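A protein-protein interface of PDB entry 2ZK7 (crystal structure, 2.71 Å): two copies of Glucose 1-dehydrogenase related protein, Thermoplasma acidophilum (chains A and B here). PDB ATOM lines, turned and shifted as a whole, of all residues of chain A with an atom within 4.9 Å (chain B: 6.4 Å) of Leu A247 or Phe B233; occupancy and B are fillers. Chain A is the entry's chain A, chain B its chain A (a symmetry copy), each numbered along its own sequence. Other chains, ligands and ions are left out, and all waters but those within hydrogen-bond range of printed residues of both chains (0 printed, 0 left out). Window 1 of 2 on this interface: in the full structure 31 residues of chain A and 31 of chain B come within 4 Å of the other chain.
OG of Ser A229 lies within hydrogen-bond range of OE1 of Glu B238.
The backbone carbonyl oxygen (O) of Ala A179 sits at hydrogen-bond distance from the backbone NH (N) of Leu A247 (2.6 Å). O of Cys A181 lies within hydrogen-bond range of N of Val A249, at 3.1 Å. O of Ile B242 sits close to NH1 of Arg B176 (3.4 Å). The backbone carbonyl oxygen of Phe B233 lies within hydrogen-bond range of the side-chain hydroxyl of Ser B236, 2.8 Å away. N of Glu B238 lies close to OG of Ser B236 (3.1 Å). SG of Cys A246 is disulfide-bonded to SG of Cys A181 (2.0 Å).
Among the printed residues, merely in contact across the chains: Ala A230 with Phe B233, Phe A233 with Ala B230, Phe A233 with Phe B233, Phe A233 with Leu B247, Leu A247 with Phe B233, Tyr A248 with Ile B242, Tyr A248 with Thr B245 and Val A249 with Ile B242.
Of the printed residues of chain B, Leu A247 touches Phe B233. Of the printed residues of chain B, Val A249 touches Ile B242. Of the printed residues of chain B, Ser A229 touches Glu B238. Of the printed residues of chain A, Thr B245 touches Tyr A248 (3.8 Å). Val B231 touches none of the printed residues of chain A.
Of the 22 printed residues of chain B, 6 touch a printed residue of chain A. Printed residues of chain B that touch a printed residue of chain A: Ala B230, Phe B233, Glu B238, Ile B242, Thr B245 and Leu B247. Hydrophobic or aromatic side chains of chain A within 4 Å of the printed part of chain B: Phe A233, Leu A247, Tyr A248 and Val A249. Among the printed residues, 9 pairs touch across the chains.
Ala A230 touches Phe B233, and with the chains exchanged Phe A233 touches Ala B230. Phe B233 touches its own counterpart, Phe A233. Phe A233 touches Leu B247, and with the chains exchanged Leu A247 touches Phe B233. 7 positions are printed for both chains.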
ATOM      1  N   ALA A 179      -5.721  -3.122 -34.400  1.00  0.00           N
ATOM      2  CA  ALA A 179      -4.517  -2.582 -33.774  1.00  0.00           C
ATOM      3  C   ALA A 179      -4.088  -3.385 -32.558  1.00  0.00           C
ATOM      4  O   ALA A 179      -4.919  -3.863 -31.785  1.00  0.00           O
ATOM      5  CB  ALA A 179      -4.704  -1.107 -33.414  1.00  0.00           C
ATOM      6  N   VAL A 180      -2.776  -3.539 -32.413  1.00  0.00           N
ATOM      7  CA  VAL A 180      -2.166  -4.124 -31.223  1.00  0.00           C
ATOM      8  C   VAL A 180      -1.532  -2.974 -30.455  1.00  0.00           C
ATOM      9  O   VAL A 180      -0.739  -2.217 -31.012  1.00  0.00           O
ATOM     10  CB  VAL A 180      -1.118  -5.214 -31.594  1.00  0.00           C
ATOM     11  CG1 VAL A 180      -0.188  -5.534 -30.429  1.00  0.00           C
ATOM     12  CG2 VAL A 180      -1.821  -6.470 -32.053  1.00  0.00           C
ATOM     13  N   CYS A 181      -1.919  -2.831 -29.190  1.00  0.00           N
ATOM     14  CA  CYS A 181      -1.424  -1.765 -28.336  1.00  0.00           C
ATOM     15  C   CYS A 181      -0.576  -2.378 -27.211  1.00  0.00           C
ATOM     16  O   CYS A 181      -1.100  -2.734 -26.149  1.00  0.00           O
ATOM     17  CB  CYS A 181      -2.596  -0.952 -27.748  1.00  0.00           C
ATOM     18  SG  CYS A 181      -3.726  -0.064 -28.915  1.00  0.00           S
ATOM     19  N   SER A 229       2.215 -12.935 -30.919  1.00  0.00           N
ATOM     20  CA  SER A 229       1.060 -13.832 -30.819  1.00  0.00           C
ATOM     21  C   SER A 229      -0.238 -13.143 -31.197  1.00  0.00           C
ATOM     22  O   SER A 229      -1.043 -13.695 -31.940  1.00  0.00           O
ATOM     23  CB  SER A 229       0.939 -14.413 -29.414  1.00  0.00           C
ATOM     24  OG  SER A 229       1.975 -15.341 -29.175  1.00  0.00           O
ATOM     25  N   ALA A 230      -0.435 -11.936 -30.674  1.00  0.00           N
ATOM     26  CA  ALA A 230      -1.648 -11.172 -30.918  1.00  0.00           C
ATOM     27  C   ALA A 230      -1.736 -10.755 -32.382  1.00  0.00           C
ATOM     28  O   ALA A 230      -2.806 -10.820 -32.997  1.00  0.00           O
ATOM     29  CB  ALA A 230      -1.695  -9.952 -30.013  1.00  0.00           C
ATOM     30  N   PHE A 233      -2.707 -13.747 -34.375  1.00  0.00           N
ATOM     31  CA  PHE A 233      -4.119 -14.027 -34.165  1.00  0.00           C
ATOM     32  C   PHE A 233      -4.966 -13.110 -35.055  1.00  0.00           C
ATOM     33  O   PHE A 233      -5.790 -13.595 -35.825  1.00  0.00           O
ATOM     34  CB  PHE A 233      -4.491 -13.894 -32.684  1.00  0.00           C
ATOM     35  CG  PHE A 233      -5.973 -13.900 -32.421  1.00  0.00           C
ATOM     36  CD1 PHE A 233      -6.639 -12.717 -32.077  1.00  0.00           C
ATOM     37  CD2 PHE A 233      -6.710 -15.076 -32.514  1.00  0.00           C
ATOM     38  CE1 PHE A 233      -8.014 -12.715 -31.833  1.00  0.00           C
ATOM     39  CE2 PHE A 233      -8.084 -15.083 -32.276  1.00  0.00           C
ATOM     40  CZ  PHE A 233      -8.735 -13.902 -31.934  1.00  0.00           C
ATOM     41  N   LEU A 234      -4.726 -11.801 -34.970  1.00  0.00           N
ATOM     42  CA  LEU A 234      -5.527 -10.802 -35.694  1.00  0.00           C
ATOM     43  C   LEU A 234      -5.372 -10.852 -37.218  1.00  0.00           C
ATOM     44  O   LEU A 234      -6.219 -10.337 -37.952  1.00  0.00           O
ATOM     45  CB  LEU A 234      -5.209  -9.388 -35.191  1.00  0.00           C
ATOM     46  CG  LEU A 234      -5.612  -9.009 -33.761  1.00  0.00           C
ATOM     47  CD1 LEU A 234      -4.977  -7.684 -33.383  1.00  0.00           C
ATOM     48  CD2 LEU A 234      -7.131  -8.960 -33.573  1.00  0.00           C
ATOM     49  N   THR A 245     -10.461  -2.710 -34.060  1.00  0.00           N
ATOM     50  CA  THR A 245     -10.373  -2.879 -32.621  1.00  0.00           C
ATOM     51  C   THR A 245      -8.907  -2.838 -32.203  1.00  0.00           C
ATOM     52  O   THR A 245      -8.034  -3.107 -33.027  1.00  0.00           O
ATOM     53  CB  THR A 245     -11.089  -4.203 -32.220  1.00  0.00           C
ATOM     54  OG1 THR A 245     -11.786  -4.030 -30.981  1.00  0.00           O
ATOM     55  CG2 THR A 245     -10.117  -5.398 -32.133  1.00  0.00           C
ATOM     56  N   CYS A 246      -8.622  -2.441 -30.962  1.00  0.00           N
ATOM     57  CA  CYS A 246      -7.244  -2.539 -30.451  1.00  0.00           C
ATOM     58  C   CYS A 246      -7.113  -3.625 -29.407  1.00  0.00           C
ATOM     59  O   CYS A 246      -7.898  -3.686 -28.461  1.00  0.00           O
ATOM     60  CB  CYS A 246      -6.595  -1.222 -29.936  1.00  0.00           C
ATOM     61  SG  CYS A 246      -4.704  -1.536 -29.925  1.00  0.00           S
ATOM     62  N   LEU A 247      -6.116  -4.478 -29.587  1.00  0.00           N
ATOM     63  CA  LEU A 247      -5.828  -5.522 -28.624  1.00  0.00           C
ATOM     64  C   LEU A 247      -4.686  -5.062 -27.752  1.00  0.00           C
ATOM     65  O   LEU A 247      -3.587  -4.772 -28.245  1.00  0.00           O
ATOM     66  CB  LEU A 247      -5.470  -6.826 -29.332  1.00  0.00           C
ATOM     67  CG  LEU A 247      -5.219  -8.097 -28.524  1.00  0.00           C
ATOM     68  CD1 LEU A 247      -6.279  -8.324 -27.437  1.00  0.00           C
ATOM     69  CD2 LEU A 247      -5.170  -9.271 -29.479  1.00  0.00           C
ATOM     70  N   TYR A 248      -4.965  -4.994 -26.454  1.00  0.00           N
ATOM     71  CA  TYR A 248      -4.016  -4.510 -25.471  1.00  0.00           C
ATOM     72  C   TYR A 248      -3.160  -5.640 -24.918  1.00  0.00           C
ATOM     73  O   TYR A 248      -3.628  -6.471 -24.137  1.00  0.00           O
ATOM     74  CB  TYR A 248      -4.747  -3.770 -24.351  1.00  0.00           C
ATOM     75  CG  TYR A 248      -5.261  -2.425 -24.796  1.00  0.00           C
ATOM     76  CD1 TYR A 248      -4.485  -1.279 -24.639  1.00  0.00           C
ATOM     77  CD2 TYR A 248      -6.514  -2.301 -25.393  1.00  0.00           C
ATOM     78  CE1 TYR A 248      -4.936  -0.043 -25.058  1.00  0.00           C
ATOM     79  CE2 TYR A 248      -6.983  -1.064 -25.817  1.00  0.00           C
ATOM     80  CZ  TYR A 248      -6.188   0.063 -25.648  1.00  0.00           C
ATOM     81  OH  TYR A 248      -6.643   1.300 -26.067  1.00  0.00           O
ATOM     82  N   VAL A 249      -1.906  -5.668 -25.352  1.00  0.00           N
ATOM     83  CA  VAL A 249      -0.910  -6.571 -24.802  1.00  0.00           C
ATOM     84  C   VAL A 249      -0.105  -5.707 -23.843  1.00  0.00           C
ATOM     85  O   VAL A 249       0.969  -5.197 -24.186  1.00  0.00           O
ATOM     86  CB  VAL A 249      -0.026  -7.185 -25.917  1.00  0.00           C
ATOM     87  CG1 VAL A 249       0.981  -8.152 -25.343  1.00  0.00           C
ATOM     88  CG2 VAL A 249      -0.889  -7.885 -26.950  1.00  0.00           C
ATOM     89  N   PHE B  10      -2.795 -24.021 -30.725  1.00  0.00           N
ATOM     90  CA  PHE B  10      -2.370 -23.817 -29.305  1.00  0.00           C
ATOM     91  C   PHE B  10      -1.873 -25.120 -28.683  1.00  0.00           C
ATOM     92  O   PHE B  10      -2.668 -25.980 -28.287  1.00  0.00           O
ATOM     93  CB  PHE B  10      -3.512 -23.233 -28.460  1.00  0.00           C
ATOM     94  CG  PHE B  10      -4.281 -22.128 -29.138  1.00  0.00           C
ATOM     95  CD1 PHE B  10      -5.542 -22.371 -29.676  1.00  0.00           C
ATOM     96  CD2 PHE B  10      -3.751 -20.844 -29.227  1.00  0.00           C
ATOM     97  CE1 PHE B  10      -6.264 -21.354 -30.298  1.00  0.00           C
ATOM     98  CE2 PHE B  10      -4.466 -19.813 -29.848  1.00  0.00           C
ATOM     99  CZ  PHE B  10      -5.724 -20.069 -30.384  1.00  0.00           C
ATOM    100  N   LEU B  13      -3.122 -25.749 -24.785  1.00  0.00           N
ATOM    101  CA  LEU B  13      -4.512 -26.026 -24.422  1.00  0.00           C
ATOM    102  C   LEU B  13      -4.815 -27.512 -24.229  1.00  0.00           C
ATOM    103  O   LEU B  13      -5.751 -27.864 -23.512  1.00  0.00           O
ATOM    104  CB  LEU B  13      -5.481 -25.411 -25.438  1.00  0.00           C
ATOM    105  CG  LEU B  13      -5.729 -23.899 -25.364  1.00  0.00           C
ATOM    106  CD1 LEU B  13      -6.809 -23.490 -26.357  1.00  0.00           C
ATOM    107  CD2 LEU B  13      -6.104 -23.442 -23.956  1.00  0.00           C
ATOM    108  N   ARG B  34     -15.000 -26.240 -29.228  1.00  0.00           N
ATOM    109  CA  ARG B  34     -13.703 -25.695 -29.646  1.00  0.00           C
ATOM    110  C   ARG B  34     -12.531 -26.210 -28.801  1.00  0.00           C
ATOM    111  O   ARG B  34     -11.491 -26.598 -29.346  1.00  0.00           O
ATOM    112  CB  ARG B  34     -13.736 -24.153 -29.654  1.00  0.00           C
ATOM    113  CG  ARG B  34     -12.430 -23.476 -30.054  1.00  0.00           C
ATOM    114  CD  ARG B  34     -11.945 -23.967 -31.401  1.00  0.00           C
ATOM    115  NE  ARG B  34     -10.536 -23.663 -31.631  1.00  0.00           N
ATOM    116  CZ  ARG B  34     -10.097 -22.617 -32.322  1.00  0.00           C
ATOM    117  NH1 ARG B  34     -10.958 -21.755 -32.853  1.00  0.00           N
ATOM    118  NH2 ARG B  34      -8.793 -22.431 -32.482  1.00  0.00           N
ATOM    119  N   PHE B  35     -12.697 -26.204 -27.480  1.00  0.00           N
ATOM    120  CA  PHE B  35     -11.684 -26.750 -26.584  1.00  0.00           C
ATOM    121  C   PHE B  35     -11.543 -28.263 -26.774  1.00  0.00           C
ATOM    122  O   PHE B  35     -10.435 -28.797 -26.736  1.00  0.00           O
ATOM    123  CB  PHE B  35     -11.986 -26.395 -25.120  1.00  0.00           C
ATOM    124  CG  PHE B  35     -11.757 -24.936 -24.779  1.00  0.00           C
ATOM    125  CD1 PHE B  35     -12.835 -24.080 -24.565  1.00  0.00           C
ATOM    126  CD2 PHE B  35     -10.466 -24.423 -24.669  1.00  0.00           C
ATOM    127  CE1 PHE B  35     -12.630 -22.735 -24.250  1.00  0.00           C
ATOM    128  CE2 PHE B  35     -10.248 -23.081 -24.349  1.00  0.00           C
ATOM    129  CZ  PHE B  35     -11.331 -22.232 -24.143  1.00  0.00           C
ATOM    130  N   ARG B 176      -5.039 -14.681 -15.186  1.00  0.00           N
ATOM    131  CA  ARG B 176      -5.522 -13.722 -16.186  1.00  0.00           C
ATOM    132  C   ARG B 176      -7.033 -13.807 -16.325  1.00  0.00           C
ATOM    133  O   ARG B 176      -7.611 -14.884 -16.226  1.00  0.00           O
ATOM    134  CB  ARG B 176      -4.892 -13.988 -17.551  1.00  0.00           C
ATOM    135  CG  ARG B 176      -3.418 -13.640 -17.669  1.00  0.00           C
ATOM    136  CD  ARG B 176      -2.878 -13.939 -19.066  1.00  0.00           C
ATOM    137  NE  ARG B 176      -3.136 -15.320 -19.484  1.00  0.00           N
ATOM    138  CZ  ARG B 176      -4.008 -15.687 -20.424  1.00  0.00           C
ATOM    139  NH1 ARG B 176      -4.728 -14.781 -21.072  1.00  0.00           N
ATOM    140  NH2 ARG B 176      -4.158 -16.969 -20.719  1.00  0.00           N
ATOM    141  N   ALA B 228     -15.889 -18.584 -30.462  1.00  0.00           N
ATOM    142  CA  ALA B 228     -15.085 -19.674 -29.915  1.00  0.00           C
ATOM    143  C   ALA B 228     -13.588 -19.517 -30.186  1.00  0.00           C
ATOM    144  O   ALA B 228     -12.767 -19.975 -29.389  1.00  0.00           O
ATOM    145  CB  ALA B 228     -15.583 -21.011 -30.437  1.00  0.00           C
ATOM    146  N   SER B 229     -13.236 -18.866 -31.295  1.00  0.00           N
ATOM    147  CA  SER B 229     -11.831 -18.606 -31.623  1.00  0.00           C
ATOM    148  C   SER B 229     -11.184 -17.635 -30.651  1.00  0.00           C
ATOM    149  O   SER B 229     -10.072 -17.867 -30.189  1.00  0.00           O
ATOM    150  CB  SER B 229     -11.691 -18.073 -33.045  1.00  0.00           C
ATOM    151  OG  SER B 229     -11.963 -19.093 -33.981  1.00  0.00           O
ATOM    152  N   ALA B 230     -11.889 -16.547 -30.353  1.00  0.00           N
ATOM    153  CA  ALA B 230     -11.381 -15.513 -29.466  1.00  0.00           C
ATOM    154  C   ALA B 230     -11.249 -16.043 -28.042  1.00  0.00           C
ATOM    155  O   ALA B 230     -10.262 -15.767 -27.351  1.00  0.00           O
ATOM    156  CB  ALA B 230     -12.291 -14.296 -29.499  1.00  0.00           C
ATOM    157  N   VAL B 231     -12.244 -16.814 -27.614  1.00  0.00           N
ATOM    158  CA  VAL B 231     -12.234 -17.410 -26.288  1.00  0.00           C
ATOM    159  C   VAL B 231     -11.020 -18.337 -26.148  1.00  0.00           C
ATOM    160  O   VAL B 231     -10.311 -18.276 -25.146  1.00  0.00           O
ATOM    161  CB  VAL B 231     -13.555 -18.158 -25.992  1.00  0.00           C
ATOM    162  CG1 VAL B 231     -13.558 -18.715 -24.572  1.00  0.00           C
ATOM    163  CG2 VAL B 231     -14.757 -17.236 -26.217  1.00  0.00           C
ATOM    164  N   ALA B 232     -10.769 -19.164 -27.163  1.00  0.00           N
ATOM    165  CA  ALA B 232      -9.633 -20.090 -27.148  1.00  0.00           C
ATOM    166  C   ALA B 232      -8.290 -19.357 -27.189  1.00  0.00           C
ATOM    167  O   ALA B 232      -7.310 -19.803 -26.577  1.00  0.00           O
ATOM    168  CB  ALA B 232      -9.728 -21.079 -28.286  1.00  0.00           C
ATOM    169  N   PHE B 233      -8.243 -18.235 -27.904  1.00  0.00           N
ATOM    170  CA  PHE B 233      -7.046 -17.410 -27.919  1.00  0.00           C
ATOM    171  C   PHE B 233      -6.769 -16.875 -26.510  1.00  0.00           C
ATOM    172  O   PHE B 233      -5.676 -17.071 -25.983  1.00  0.00           O
ATOM    173  CB  PHE B 233      -7.168 -16.281 -28.948  1.00  0.00           C
ATOM    174  CG  PHE B 233      -6.096 -15.230 -28.837  1.00  0.00           C
ATOM    175  CD1 PHE B 233      -6.391 -13.969 -28.306  1.00  0.00           C
ATOM    176  CD2 PHE B 233      -4.796 -15.490 -29.258  1.00  0.00           C
ATOM    177  CE1 PHE B 233      -5.400 -12.988 -28.200  1.00  0.00           C
ATOM    178  CE2 PHE B 233      -3.800 -14.519 -29.151  1.00  0.00           C
ATOM    179  CZ  PHE B 233      -4.104 -13.269 -28.624  1.00  0.00           C
ATOM    180  N   LEU B 234      -7.770 -16.241 -25.899  1.00  0.00           N
ATOM    181  CA  LEU B 234      -7.616 -15.595 -24.587  1.00  0.00           C
ATOM    182  C   LEU B 234      -7.369 -16.568 -23.429  1.00  0.00           C
ATOM    183  O   LEU B 234      -6.880 -16.171 -22.369  1.00  0.00           O
ATOM    184  CB  LEU B 234      -8.834 -14.717 -24.270  1.00  0.00           C
ATOM    185  CG  LEU B 234      -9.073 -13.460 -25.115  1.00  0.00           C
ATOM    186  CD1 LEU B 234     -10.448 -12.897 -24.817  1.00  0.00           C
ATOM    187  CD2 LEU B 234      -7.990 -12.398 -24.905  1.00  0.00           C
ATOM    188  N   ALA B 235      -7.707 -17.838 -23.638  1.00  0.00           N
ATOM    189  CA  ALA B 235      -7.544 -18.865 -22.616  1.00  0.00           C
ATOM    190  C   ALA B 235      -6.178 -19.531 -22.711  1.00  0.00           C
ATOM    191  O   ALA B 235      -5.708 -20.135 -21.746  1.00  0.00           O
ATOM    192  CB  ALA B 235      -8.642 -19.897 -22.732  1.00  0.00           C
ATOM    193  N   SER B 236      -5.544 -19.415 -23.873  1.00  0.00           N
ATOM    194  CA  SER B 236      -4.272 -20.074 -24.131  1.00  0.00           C
ATOM    195  C   SER B 236      -3.096 -19.223 -23.685  1.00  0.00           C
ATOM    196  O   SER B 236      -3.267 -18.059 -23.334  1.00  0.00           O
ATOM    197  CB  SER B 236      -4.128 -20.364 -25.624  1.00  0.00           C
ATOM    198  OG  SER B 236      -3.838 -19.170 -26.329  1.00  0.00           O
ATOM    199  N   ARG B 237      -1.904 -19.810 -23.742  1.00  0.00           N
ATOM    200  CA  ARG B 237      -0.658 -19.117 -23.436  1.00  0.00           C
ATOM    201  C   ARG B 237      -0.333 -18.024 -24.459  1.00  0.00           C
ATOM    202  O   ARG B 237       0.501 -17.152 -24.206  1.00  0.00           O
ATOM    203  CB  ARG B 237       0.499 -20.128 -23.340  1.00  0.00           C
ATOM    204  CG  ARG B 237       1.764 -19.615 -22.639  1.00  0.00           C
ATOM    205  CD  ARG B 237       1.469 -19.118 -21.220  1.00  0.00           C
ATOM    206  NE  ARG B 237       2.683 -18.809 -20.462  1.00  0.00           N
ATOM    207  CZ  ARG B 237       2.709 -18.146 -19.304  1.00  0.00           C
ATOM    208  NH1 ARG B 237       3.870 -17.925 -18.693  1.00  0.00           N
ATOM    209  NH2 ARG B 237       1.580 -17.699 -18.754  1.00  0.00           N
ATOM    210  N   GLU B 238      -0.994 -18.068 -25.614  1.00  0.00           N
ATOM    211  CA  GLU B 238      -0.817 -17.036 -26.639  1.00  0.00           C
ATOM    212  C   GLU B 238      -1.117 -15.636 -26.106  1.00  0.00           C
ATOM    213  O   GLU B 238      -0.459 -14.671 -26.504  1.00  0.00           O
ATOM    214  CB  GLU B 238      -1.682 -17.328 -27.871  1.00  0.00           C
ATOM    215  CG  GLU B 238      -1.240 -18.547 -28.663  1.00  0.00           C
ATOM    216  CD  GLU B 238       0.038 -18.309 -29.441  1.00  0.00           C
ATOM    217  OE1 GLU B 238       0.006 -17.534 -30.424  1.00  0.00           O
ATOM    218  OE2 GLU B 238       1.075 -18.903 -29.077  1.00  0.00           O
ATOM    219  N   ALA B 239      -2.095 -15.541 -25.203  1.00  0.00           N
ATOM    220  CA  ALA B 239      -2.496 -14.272 -24.602  1.00  0.00           C
ATOM    221  C   ALA B 239      -1.889 -14.057 -23.221  1.00  0.00           C
ATOM    222  O   ALA B 239      -2.456 -13.347 -22.392  1.00  0.00           O
ATOM    223  CB  ALA B 239      -4.017 -14.195 -24.521  1.00  0.00           C
ATOM    224  N   SER B 240      -0.728 -14.656 -22.979  1.00  0.00           N
ATOM    225  CA  SER B 240      -0.088 -14.632 -21.657  1.00  0.00           C
ATOM    226  C   SER B 240       0.162 -13.248 -21.037  1.00  0.00           C
ATOM    227  O   SER B 240       0.404 -13.158 -19.832  1.00  0.00           O
ATOM    228  CB  SER B 240       1.228 -15.399 -21.693  1.00  0.00           C
ATOM    229  OG  SER B 240       2.102 -14.829 -22.648  1.00  0.00           O
ATOM    230  N   ILE B 242      -1.990 -10.615 -21.884  1.00  0.00           N
ATOM    231  CA  ILE B 242      -3.265  -9.950 -22.060  1.00  0.00           C
ATOM    232  C   ILE B 242      -4.165 -10.254 -20.869  1.00  0.00           C
ATOM    233  O   ILE B 242      -4.451 -11.423 -20.579  1.00  0.00           O
ATOM    234  CB  ILE B 242      -3.957 -10.397 -23.373  1.00  0.00           C
ATOM    235  CG1 ILE B 242      -3.073 -10.079 -24.586  1.00  0.00           C
ATOM    236  CG2 ILE B 242      -5.331  -9.752 -23.509  1.00  0.00           C
ATOM    237  CD1 ILE B 242      -3.514 -10.776 -25.860  1.00  0.00           C
ATOM    238  N   THR B 245      -9.181  -7.131 -20.298  1.00  0.00           N
ATOM    239  CA  THR B 245      -9.460  -6.476 -21.563  1.00  0.00           C
ATOM    240  C   THR B 245     -10.690  -7.118 -22.196  1.00  0.00           C
ATOM    241  O   THR B 245     -11.008  -8.263 -21.878  1.00  0.00           O
ATOM    242  CB  THR B 245      -8.193  -6.555 -22.466  1.00  0.00           C
ATOM    243  OG1 THR B 245      -8.041  -5.340 -23.208  1.00  0.00           O
ATOM    244  CG2 THR B 245      -8.219  -7.771 -23.415  1.00  0.00           C
ATOM    245  N   CYS B 246     -11.421  -6.377 -23.031  1.00  0.00           N
ATOM    246  CA  CYS B 246     -12.520  -6.991 -23.796  1.00  0.00           C
ATOM    247  C   CYS B 246     -12.184  -7.097 -25.266  1.00  0.00           C
ATOM    248  O   CYS B 246     -11.757  -6.122 -25.886  1.00  0.00           O
ATOM    249  CB  CYS B 246     -13.932  -6.364 -23.615  1.00  0.00           C
ATOM    250  SG  CYS B 246     -15.179  -7.691 -24.213  1.00  0.00           S
ATOM    251  N   LEU B 247     -12.379  -8.286 -25.816  1.00  0.00           N
ATOM    252  CA  LEU B 247     -12.169  -8.509 -27.233  1.00  0.00           C
ATOM    253  C   LEU B 247     -13.510  -8.464 -27.924  1.00  0.00           C
ATOM    254  O   LEU B 247     -14.414  -9.250 -27.609  1.00  0.00           O
ATOM    255  CB  LEU B 247     -11.487  -9.853 -27.472  1.00  0.00           C
ATOM    256  CG  LEU B 247     -11.077 -10.267 -28.884  1.00  0.00           C
ATOM    257  CD1 LEU B 247     -10.371  -9.139 -29.648  1.00  0.00           C
ATOM    258  CD2 LEU B 247     -10.186 -11.488 -28.785  1.00  0.00           C
